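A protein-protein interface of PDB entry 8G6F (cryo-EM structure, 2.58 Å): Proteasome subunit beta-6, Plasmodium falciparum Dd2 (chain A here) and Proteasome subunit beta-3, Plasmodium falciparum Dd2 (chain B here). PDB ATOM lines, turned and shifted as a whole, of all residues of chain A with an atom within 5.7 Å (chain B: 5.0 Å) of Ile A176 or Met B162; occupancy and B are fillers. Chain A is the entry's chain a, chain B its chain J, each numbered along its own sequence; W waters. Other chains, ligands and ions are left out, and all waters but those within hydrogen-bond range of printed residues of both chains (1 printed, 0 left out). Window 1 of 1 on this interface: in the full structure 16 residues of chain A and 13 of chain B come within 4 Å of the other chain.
The side-chain hydroxyl (OG) of Ser B165 is in hydrogen-bond range of the side-chain carboxylate (OD2) of Asp A204, at 2.8 Å. The side-chain amide oxygen (OE1) of Gln B182 sits at hydrogen-bond distance from the side-chain amide nitrogen (ND2) of Asn A179. The backbone NH (N) of Ile A176 sits at hydrogen-bond distance from the side-chain sulfur (SD) of Met B162, 3.7 Å away. The side-chain amide nitrogen (ND2) of Asn A179 lies within hydrogen-bond range of the side-chain hydroxyl (OG) of Ser B186 (2.9 Å). The side-chain sulfur (SD) of Met B162 sits close to the backbone carbonyl oxygen (O) of Pro A175. OG of Ser A208 lies within hydrogen-bond range of OG of Ser B165.
The side-chain hydroxyl of Ser A208 is in hydrogen-bond range of the backbone carbonyl oxygen of Asp A204. O of Met B162 is in hydrogen-bond range of SG of Cys B183, 3.8 Å away. The side-chain carboxylate (OD2) of Asp A204 lies within salt-bridge range of the guanidinium group (NH2) of Arg A180, 3.9 Å away. The backbone carbonyl oxygen (O) of Gln B182 lies within hydrogen-bond range of the side-chain hydroxyl (OG) of Ser B186 (3.0 Å).
O of Leu A172 touches CA of Gly B161 (3.6 Å). Pro A175 touches Gln B158. O of Ser B186 touches CB of Pro A175 (3.9 Å). Ile A176 touches Gly B161 (CD1 to O, 3.3 Å). Ser B165 touches Ile A176. Arg A180 touches Ser B165. Arg A180 touches Leu B166 (NH2 to CD2, 3.8 Å). Ser A208 touches Glu B164 (OG to C, 3.9 Å).
Ile A176 touches three residues of chain B. Of the printed residues of chain A, Met B162 touches Pro A175 and Ile A176. Of the printed residues of chain A, Leu B166 touches Arg A180. Of the printed residues of chain B, Leu A172 touches Gly B161 (3.6 Å). Ala A205 touches none of the printed residues of chain B. The nearest residue of chain B that does not touch Ile A176 is Leu B166 (4.7 Å). The nearest printed residue of chain B that does not touch Ser A208 is Gly B161 (4.5 Å).
Along chain B the printed residues that touch a printed residue of chain A span positions 158 to 186. Of the 14 printed residues of chain A, 7 touch a printed residue of chain B. Printed residues of chain A that touch a printed residue of chain B: Leu A172, Pro A175, Ile A176, Asn A179, Arg A180, Asp A204 and Ser A208. Among the printed residues, 14 pairs touch across the chains. Among the printed residues, no Asp or Glu carboxylate lies within 4 Å of a Lys or Arg side-chain nitrogen of the other chain.
Water W1 lies within hydrogen-bond range of O of Ser B186 (2.8 Å) and OD2 of Asp A178 (3.1 Å).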
ATOM      1  N   LEU A 172       5.262  -0.825   1.037  1.00  0.00           N
ATOM      2  CA  LEU A 172       4.962  -0.999  -0.376  1.00  0.00           C
ATOM      3  C   LEU A 172       5.519   0.145  -1.213  1.00  0.00           C
ATOM      4  O   LEU A 172       5.991  -0.075  -2.331  1.00  0.00           O
ATOM      5  CB  LEU A 172       3.453  -1.106  -0.589  1.00  0.00           C
ATOM      6  CG  LEU A 172       2.732  -2.299   0.033  1.00  0.00           C
ATOM      7  CD1 LEU A 172       1.784  -1.845   1.118  1.00  0.00           C
ATOM      8  CD2 LEU A 172       1.983  -3.073  -1.027  1.00  0.00           C
ATOM      9  N   ILE A 173       5.480   1.366  -0.688  1.00  0.00           N
ATOM     10  CA  ILE A 173       5.744   2.547  -1.503  1.00  0.00           C
ATOM     11  C   ILE A 173       7.228   2.881  -1.568  1.00  0.00           C
ATOM     12  O   ILE A 173       7.739   3.223  -2.634  1.00  0.00           O
ATOM     13  CB  ILE A 173       4.924   3.734  -0.966  1.00  0.00           C
ATOM     14  CG1 ILE A 173       3.461   3.573  -1.366  1.00  0.00           C
ATOM     15  CG2 ILE A 173       5.472   5.043  -1.495  1.00  0.00           C
ATOM     16  CD1 ILE A 173       2.513   4.403  -0.555  1.00  0.00           C
ATOM     17  N   LEU A 174       7.943   2.809  -0.448  1.00  0.00           N
ATOM     18  CA  LEU A 174       9.330   3.262  -0.436  1.00  0.00           C
ATOM     19  C   LEU A 174      10.197   2.579  -1.486  1.00  0.00           C
ATOM     20  O   LEU A 174      11.015   3.274  -2.113  1.00  0.00           O
ATOM     21  CB  LEU A 174       9.919   3.073   0.965  1.00  0.00           C
ATOM     22  CG  LEU A 174       9.430   4.080   2.006  1.00  0.00           C
ATOM     23  CD1 LEU A 174       9.752   3.604   3.404  1.00  0.00           C
ATOM     24  CD2 LEU A 174      10.035   5.452   1.757  1.00  0.00           C
ATOM     25  N   PRO A 175      10.106   1.265  -1.712  1.00  0.00           N
ATOM     26  CA  PRO A 175      10.885   0.669  -2.809  1.00  0.00           C
ATOM     27  C   PRO A 175      10.603   1.298  -4.160  1.00  0.00           C
ATOM     28  O   PRO A 175      11.529   1.497  -4.956  1.00  0.00           O
ATOM     29  CB  PRO A 175      10.459  -0.803  -2.776  1.00  0.00           C
ATOM     30  CG  PRO A 175       9.970  -1.033  -1.407  1.00  0.00           C
ATOM     31  CD  PRO A 175       9.386   0.248  -0.930  1.00  0.00           C
ATOM     32  N   ILE A 176       9.340   1.622  -4.442  1.00  0.00           N
ATOM     33  CA  ILE A 176       8.991   2.215  -5.730  1.00  0.00           C
ATOM     34  C   ILE A 176       9.679   3.559  -5.893  1.00  0.00           C
ATOM     35  O   ILE A 176      10.261   3.860  -6.941  1.00  0.00           O
ATOM     36  CB  ILE A 176       7.465   2.359  -5.856  1.00  0.00           C
ATOM     37  CG1 ILE A 176       6.777   1.002  -5.741  1.00  0.00           C
ATOM     38  CG2 ILE A 176       7.107   3.026  -7.169  1.00  0.00           C
ATOM     39  CD1 ILE A 176       5.337   1.105  -5.323  1.00  0.00           C
ATOM     40  N   LEU A 177       9.602   4.399  -4.862  1.00  0.00           N
ATOM     41  CA  LEU A 177      10.213   5.717  -4.938  1.00  0.00           C
ATOM     42  C   LEU A 177      11.729   5.625  -4.993  1.00  0.00           C
ATOM     43  O   LEU A 177      12.372   6.450  -5.643  1.00  0.00           O
ATOM     44  CB  LEU A 177       9.763   6.561  -3.750  1.00  0.00           C
ATOM     45  CG  LEU A 177       8.251   6.766  -3.648  1.00  0.00           C
ATOM     46  CD1 LEU A 177       7.908   7.611  -2.440  1.00  0.00           C
ATOM     47  CD2 LEU A 177       7.697   7.401  -4.911  1.00  0.00           C
ATOM     48  N   ASP A 178      12.317   4.633  -4.324  1.00  0.00           N
ATOM     49  CA  ASP A 178      13.749   4.403  -4.469  1.00  0.00           C
ATOM     50  C   ASP A 178      14.099   4.065  -5.907  1.00  0.00           C
ATOM     51  O   ASP A 178      15.075   4.583  -6.457  1.00  0.00           O
ATOM     52  CB  ASP A 178      14.197   3.273  -3.545  1.00  0.00           C
ATOM     53  CG  ASP A 178      14.193   3.671  -2.095  1.00  0.00           C
ATOM     54  OD1 ASP A 178      13.855   4.832  -1.796  1.00  0.00           O
ATOM     55  OD2 ASP A 178      14.518   2.820  -1.249  1.00  0.00           O
ATOM     56  N   ASN A 179      13.310   3.193  -6.532  1.00  0.00           N
ATOM     57  CA  ASN A 179      13.577   2.799  -7.909  1.00  0.00           C
ATOM     58  C   ASN A 179      13.426   3.976  -8.863  1.00  0.00           C
ATOM     59  O   ASN A 179      14.208   4.122  -9.808  1.00  0.00           O
ATOM     60  CB  ASN A 179      12.642   1.658  -8.303  1.00  0.00           C
ATOM     61  CG  ASN A 179      12.899   1.144  -9.698  1.00  0.00           C
ATOM     62  OD1 ASN A 179      12.292   1.602 -10.662  1.00  0.00           O
ATOM     63  ND2 ASN A 179      13.799   0.181  -9.815  1.00  0.00           N
ATOM     64  N   ARG A 180      12.425   4.822  -8.636  1.00  0.00           N
ATOM     65  CA  ARG A 180      12.136   5.910  -9.563  1.00  0.00           C
ATOM     66  C   ARG A 180      13.004   7.140  -9.337  1.00  0.00           C
ATOM     67  O   ARG A 180      13.187   7.926 -10.271  1.00  0.00           O
ATOM     68  CB  ARG A 180      10.664   6.308  -9.460  1.00  0.00           C
ATOM     69  CG  ARG A 180       9.704   5.204  -9.847  1.00  0.00           C
ATOM     70  CD  ARG A 180       8.343   5.753 -10.215  1.00  0.00           C
ATOM     71  NE  ARG A 180       7.445   4.709 -10.693  1.00  0.00           N
ATOM     72  CZ  ARG A 180       7.527   4.138 -11.886  1.00  0.00           C
ATOM     73  NH1 ARG A 180       8.462   4.482 -12.755  1.00  0.00           N
ATOM     74  NH2 ARG A 180       6.646   3.200 -12.217  1.00  0.00           N
ATOM     75  N   VAL A 181      13.546   7.326  -8.136  1.00  0.00           N
ATOM     76  CA  VAL A 181      14.287   8.534  -7.781  1.00  0.00           C
ATOM     77  C   VAL A 181      15.787   8.263  -7.708  1.00  0.00           C
ATOM     78  O   VAL A 181      16.574   8.891  -8.416  1.00  0.00           O
ATOM     79  CB  VAL A 181      13.762   9.135  -6.458  1.00  0.00           C
ATOM     80  CG1 VAL A 181      14.633  10.294  -6.022  1.00  0.00           C
ATOM     81  CG2 VAL A 181      12.321   9.578  -6.616  1.00  0.00           C
ATOM     82  N   ASP A 204       1.017   7.345  -8.804  1.00  0.00           N
ATOM     83  CA  ASP A 204       1.209   5.927  -9.078  1.00  0.00           C
ATOM     84  C   ASP A 204       1.556   5.164  -7.808  1.00  0.00           C
ATOM     85  O   ASP A 204       1.057   4.058  -7.587  1.00  0.00           O
ATOM     86  CB  ASP A 204       2.301   5.740 -10.127  1.00  0.00           C
ATOM     87  CG  ASP A 204       2.564   4.281 -10.439  1.00  0.00           C
ATOM     88  OD1 ASP A 204       1.766   3.683 -11.187  1.00  0.00           O
ATOM     89  OD2 ASP A 204       3.564   3.728  -9.934  1.00  0.00           O
ATOM     90  N   ALA A 205       2.416   5.734  -6.966  1.00  0.00           N
ATOM     91  CA  ALA A 205       2.793   5.053  -5.734  1.00  0.00           C
ATOM     92  C   ALA A 205       1.590   4.851  -4.823  1.00  0.00           C
ATOM     93  O   ALA A 205       1.396   3.762  -4.271  1.00  0.00           O
ATOM     94  CB  ALA A 205       3.884   5.843  -5.012  1.00  0.00           C
ATOM     95  N   SER A 208      -0.695   2.138  -6.309  1.00  0.00           N
ATOM     96  CA  SER A 208      -0.148   0.803  -6.113  1.00  0.00           C
ATOM     97  C   SER A 208      -0.290   0.362  -4.664  1.00  0.00           C
ATOM     98  O   SER A 208      -0.586  -0.805  -4.390  1.00  0.00           O
ATOM     99  CB  SER A 208       1.315   0.767  -6.547  1.00  0.00           C
ATOM    100  OG  SER A 208       1.434   1.052  -7.926  1.00  0.00           O
ATOM    101  N   ALA A 209      -0.076   1.276  -3.719  1.00  0.00           N
ATOM    102  CA  ALA A 209      -0.298   0.935  -2.318  1.00  0.00           C
ATOM    103  C   ALA A 209      -1.761   0.599  -2.061  1.00  0.00           C
ATOM    104  O   ALA A 209      -2.067  -0.325  -1.302  1.00  0.00           O
ATOM    105  CB  ALA A 209       0.149   2.082  -1.419  1.00  0.00           C
ATOM    106  N   GLN B 158       7.382  -5.264  -0.043  1.00  0.00           N
ATOM    107  CA  GLN B 158       8.190  -4.521  -1.000  1.00  0.00           C
ATOM    108  C   GLN B 158       8.035  -5.090  -2.402  1.00  0.00           C
ATOM    109  O   GLN B 158       7.910  -4.339  -3.377  1.00  0.00           O
ATOM    110  CB  GLN B 158       9.652  -4.544  -0.568  1.00  0.00           C
ATOM    111  CG  GLN B 158       9.930  -3.785   0.712  1.00  0.00           C
ATOM    112  CD  GLN B 158       9.916  -4.669   1.939  1.00  0.00           C
ATOM    113  OE1 GLN B 158       8.930  -5.339   2.226  1.00  0.00           O
ATOM    114  NE2 GLN B 158      11.015  -4.668   2.672  1.00  0.00           N
ATOM    115  N   LEU B 159       8.041  -6.417  -2.523  1.00  0.00           N
ATOM    116  CA  LEU B 159       7.886  -7.030  -3.836  1.00  0.00           C
ATOM    117  C   LEU B 159       6.510  -6.744  -4.422  1.00  0.00           C
ATOM    118  O   LEU B 159       6.384  -6.489  -5.622  1.00  0.00           O
ATOM    119  CB  LEU B 159       8.135  -8.532  -3.739  1.00  0.00           C
ATOM    120  CG  LEU B 159       9.601  -8.936  -3.580  1.00  0.00           C
ATOM    121  CD1 LEU B 159       9.716 -10.396  -3.196  1.00  0.00           C
ATOM    122  CD2 LEU B 159      10.371  -8.654  -4.853  1.00  0.00           C
ATOM    123  N   PHE B 160       5.467  -6.780  -3.593  1.00  0.00           N
ATOM    124  CA  PHE B 160       4.126  -6.464  -4.065  1.00  0.00           C
ATOM    125  C   PHE B 160       4.054  -5.039  -4.584  1.00  0.00           C
ATOM    126  O   PHE B 160       3.476  -4.788  -5.644  1.00  0.00           O
ATOM    127  CB  PHE B 160       3.112  -6.657  -2.937  1.00  0.00           C
ATOM    128  CG  PHE B 160       2.496  -8.023  -2.888  1.00  0.00           C
ATOM    129  CD1 PHE B 160       2.012  -8.631  -4.031  1.00  0.00           C
ATOM    130  CD2 PHE B 160       2.388  -8.695  -1.687  1.00  0.00           C
ATOM    131  CE1 PHE B 160       1.445  -9.883  -3.975  1.00  0.00           C
ATOM    132  CE2 PHE B 160       1.820  -9.945  -1.630  1.00  0.00           C
ATOM    133  CZ  PHE B 160       1.349 -10.540  -2.776  1.00  0.00           C
ATOM    134  N   GLY B 161       4.634  -4.092  -3.851  1.00  0.00           N
ATOM    135  CA  GLY B 161       4.619  -2.716  -4.319  1.00  0.00           C
ATOM    136  C   GLY B 161       5.363  -2.547  -5.628  1.00  0.00           C
ATOM    137  O   GLY B 161       4.863  -1.927  -6.573  1.00  0.00           O
ATOM    138  N   MET B 162       6.566  -3.119  -5.709  1.00  0.00           N
ATOM    139  CA  MET B 162       7.362  -2.978  -6.921  1.00  0.00           C
ATOM    140  C   MET B 162       6.666  -3.613  -8.113  1.00  0.00           C
ATOM    141  O   MET B 162       6.673  -3.054  -9.213  1.00  0.00           O
ATOM    142  CB  MET B 162       8.742  -3.598  -6.714  1.00  0.00           C
ATOM    143  CG  MET B 162       9.705  -2.721  -5.931  1.00  0.00           C
ATOM    144  SD  MET B 162      10.136  -1.157  -6.714  1.00  0.00           S
ATOM    145  CE  MET B 162      10.283  -1.613  -8.432  1.00  0.00           C
ATOM    146  N   CYS B 163       6.059  -4.785  -7.921  1.00  0.00           N
ATOM    147  CA  CYS B 163       5.409  -5.472  -9.029  1.00  0.00           C
ATOM    148  C   CYS B 163       4.110  -4.794  -9.430  1.00  0.00           C
ATOM    149  O   CYS B 163       3.760  -4.784 -10.614  1.00  0.00           O
ATOM    150  CB  CYS B 163       5.154  -6.928  -8.656  1.00  0.00           C
ATOM    151  SG  CYS B 163       6.622  -7.965  -8.667  1.00  0.00           S
ATOM    152  N   GLU B 164       3.374  -4.233  -8.470  1.00  0.00           N
ATOM    153  CA  GLU B 164       2.184  -3.471  -8.818  1.00  0.00           C
ATOM    154  C   GLU B 164       2.549  -2.247  -9.640  1.00  0.00           C
ATOM    155  O   GLU B 164       1.832  -1.887 -10.580  1.00  0.00           O
ATOM    156  CB  GLU B 164       1.432  -3.055  -7.554  1.00  0.00           C
ATOM    157  CG  GLU B 164       0.647  -4.175  -6.900  1.00  0.00           C
ATOM    158  CD  GLU B 164      -0.465  -4.691  -7.777  1.00  0.00           C
ATOM    159  OE1 GLU B 164      -0.784  -4.025  -8.782  1.00  0.00           O
ATOM    160  OE2 GLU B 164      -1.023  -5.762  -7.466  1.00  0.00           O
ATOM    161  N   SER B 165       3.657  -1.590  -9.301  1.00  0.00           N
ATOM    162  CA  SER B 165       4.014  -0.373 -10.015  1.00  0.00           C
ATOM    163  C   SER B 165       4.688  -0.638 -11.354  1.00  0.00           C
ATOM    164  O   SER B 165       4.466   0.118 -12.304  1.00  0.00           O
ATOM    165  CB  SER B 165       4.919   0.493  -9.143  1.00  0.00           C
ATOM    166  OG  SER B 165       4.152   1.450  -8.441  1.00  0.00           O
ATOM    167  N   LEU B 166       5.504  -1.688 -11.466  1.00  0.00           N
ATOM    168  CA  LEU B 166       6.420  -1.817 -12.589  1.00  0.00           C
ATOM    169  C   LEU B 166       6.109  -2.963 -13.540  1.00  0.00           C
ATOM    170  O   LEU B 166       6.644  -2.972 -14.650  1.00  0.00           O
ATOM    171  CB  LEU B 166       7.860  -1.993 -12.081  1.00  0.00           C
ATOM    172  CG  LEU B 166       8.696  -0.731 -11.837  1.00  0.00           C
ATOM    173  CD1 LEU B 166       8.794   0.129 -13.084  1.00  0.00           C
ATOM    174  CD2 LEU B 166       8.140   0.080 -10.684  1.00  0.00           C
ATOM    175  N   TYR B 167       5.275  -3.923 -13.150  1.00  0.00           N
ATOM    176  CA  TYR B 167       4.988  -5.043 -14.036  1.00  0.00           C
ATOM    177  C   TYR B 167       4.336  -4.552 -15.320  1.00  0.00           C
ATOM    178  O   TYR B 167       3.423  -3.724 -15.290  1.00  0.00           O
ATOM    179  CB  TYR B 167       4.082  -6.061 -13.348  1.00  0.00           C
ATOM    180  CG  TYR B 167       3.557  -7.111 -14.302  1.00  0.00           C
ATOM    181  CD1 TYR B 167       4.324  -8.217 -14.639  1.00  0.00           C
ATOM    182  CD2 TYR B 167       2.305  -6.985 -14.880  1.00  0.00           C
ATOM    183  CE1 TYR B 167       3.854  -9.166 -15.514  1.00  0.00           C
ATOM    184  CE2 TYR B 167       1.829  -7.931 -15.758  1.00  0.00           C
ATOM    185  CZ  TYR B 167       2.608  -9.016 -16.073  1.00  0.00           C
ATOM    186  OH  TYR B 167       2.133  -9.960 -16.947  1.00  0.00           O
ATOM    187  N   GLN B 182      14.868  -5.669 -11.677  1.00  0.00           N
ATOM    188  CA  GLN B 182      14.704  -4.372 -11.033  1.00  0.00           C
ATOM    189  C   GLN B 182      13.776  -4.471  -9.833  1.00  0.00           C
ATOM    190  O   GLN B 182      14.066  -3.914  -8.766  1.00  0.00           O
ATOM    191  CB  GLN B 182      14.173  -3.354 -12.039  1.00  0.00           C
ATOM    192  CG  GLN B 182      15.230  -2.805 -12.981  1.00  0.00           C
ATOM    193  CD  GLN B 182      16.418  -2.235 -12.250  1.00  0.00           C
ATOM    194  OE1 GLN B 182      16.268  -1.584 -11.221  1.00  0.00           O
ATOM    195  NE2 GLN B 182      17.607  -2.480 -12.771  1.00  0.00           N
ATOM    196  N   CYS B 183      12.659  -5.181  -9.985  1.00  0.00           N
ATOM    197  CA  CYS B 183      11.748  -5.372  -8.864  1.00  0.00           C
ATOM    198  C   CYS B 183      12.464  -6.030  -7.694  1.00  0.00           C
ATOM    199  O   CYS B 183      12.381  -5.558  -6.554  1.00  0.00           O
ATOM    200  CB  CYS B 183      10.551  -6.215  -9.305  1.00  0.00           C
ATOM    201  SG  CYS B 183       9.403  -5.380 -10.414  1.00  0.00           S
ATOM    202  N   SER B 186      15.212  -3.633  -6.060  1.00  0.00           N
ATOM    203  CA  SER B 186      14.631  -2.541  -5.292  1.00  0.00           C
ATOM    204  C   SER B 186      13.960  -3.051  -4.024  1.00  0.00           C
ATOM    205  O   SER B 186      14.042  -2.405  -2.975  1.00  0.00           O
ATOM    206  CB  SER B 186      13.639  -1.774  -6.156  1.00  0.00           C
ATOM    207  OG  SER B 186      14.284  -1.251  -7.299  1.00  0.00           O
ATOM    208  N   ALA B 187      13.286  -4.202  -4.097  1.00  0.00           N
ATOM    209  CA  ALA B 187      12.660  -4.753  -2.900  1.00  0.00           C
ATOM    210  C   ALA B 187      13.704  -5.217  -1.893  1.00  0.00           C
ATOM    211  O   ALA B 187      13.523  -5.048  -0.684  1.00  0.00           O
ATOM    212  CB  ALA B 187      11.731  -5.901  -3.280  1.00  0.00           C
HETATM  213  O   HOH W   1      15.045   0.155  -2.782  1.00  0.00           O
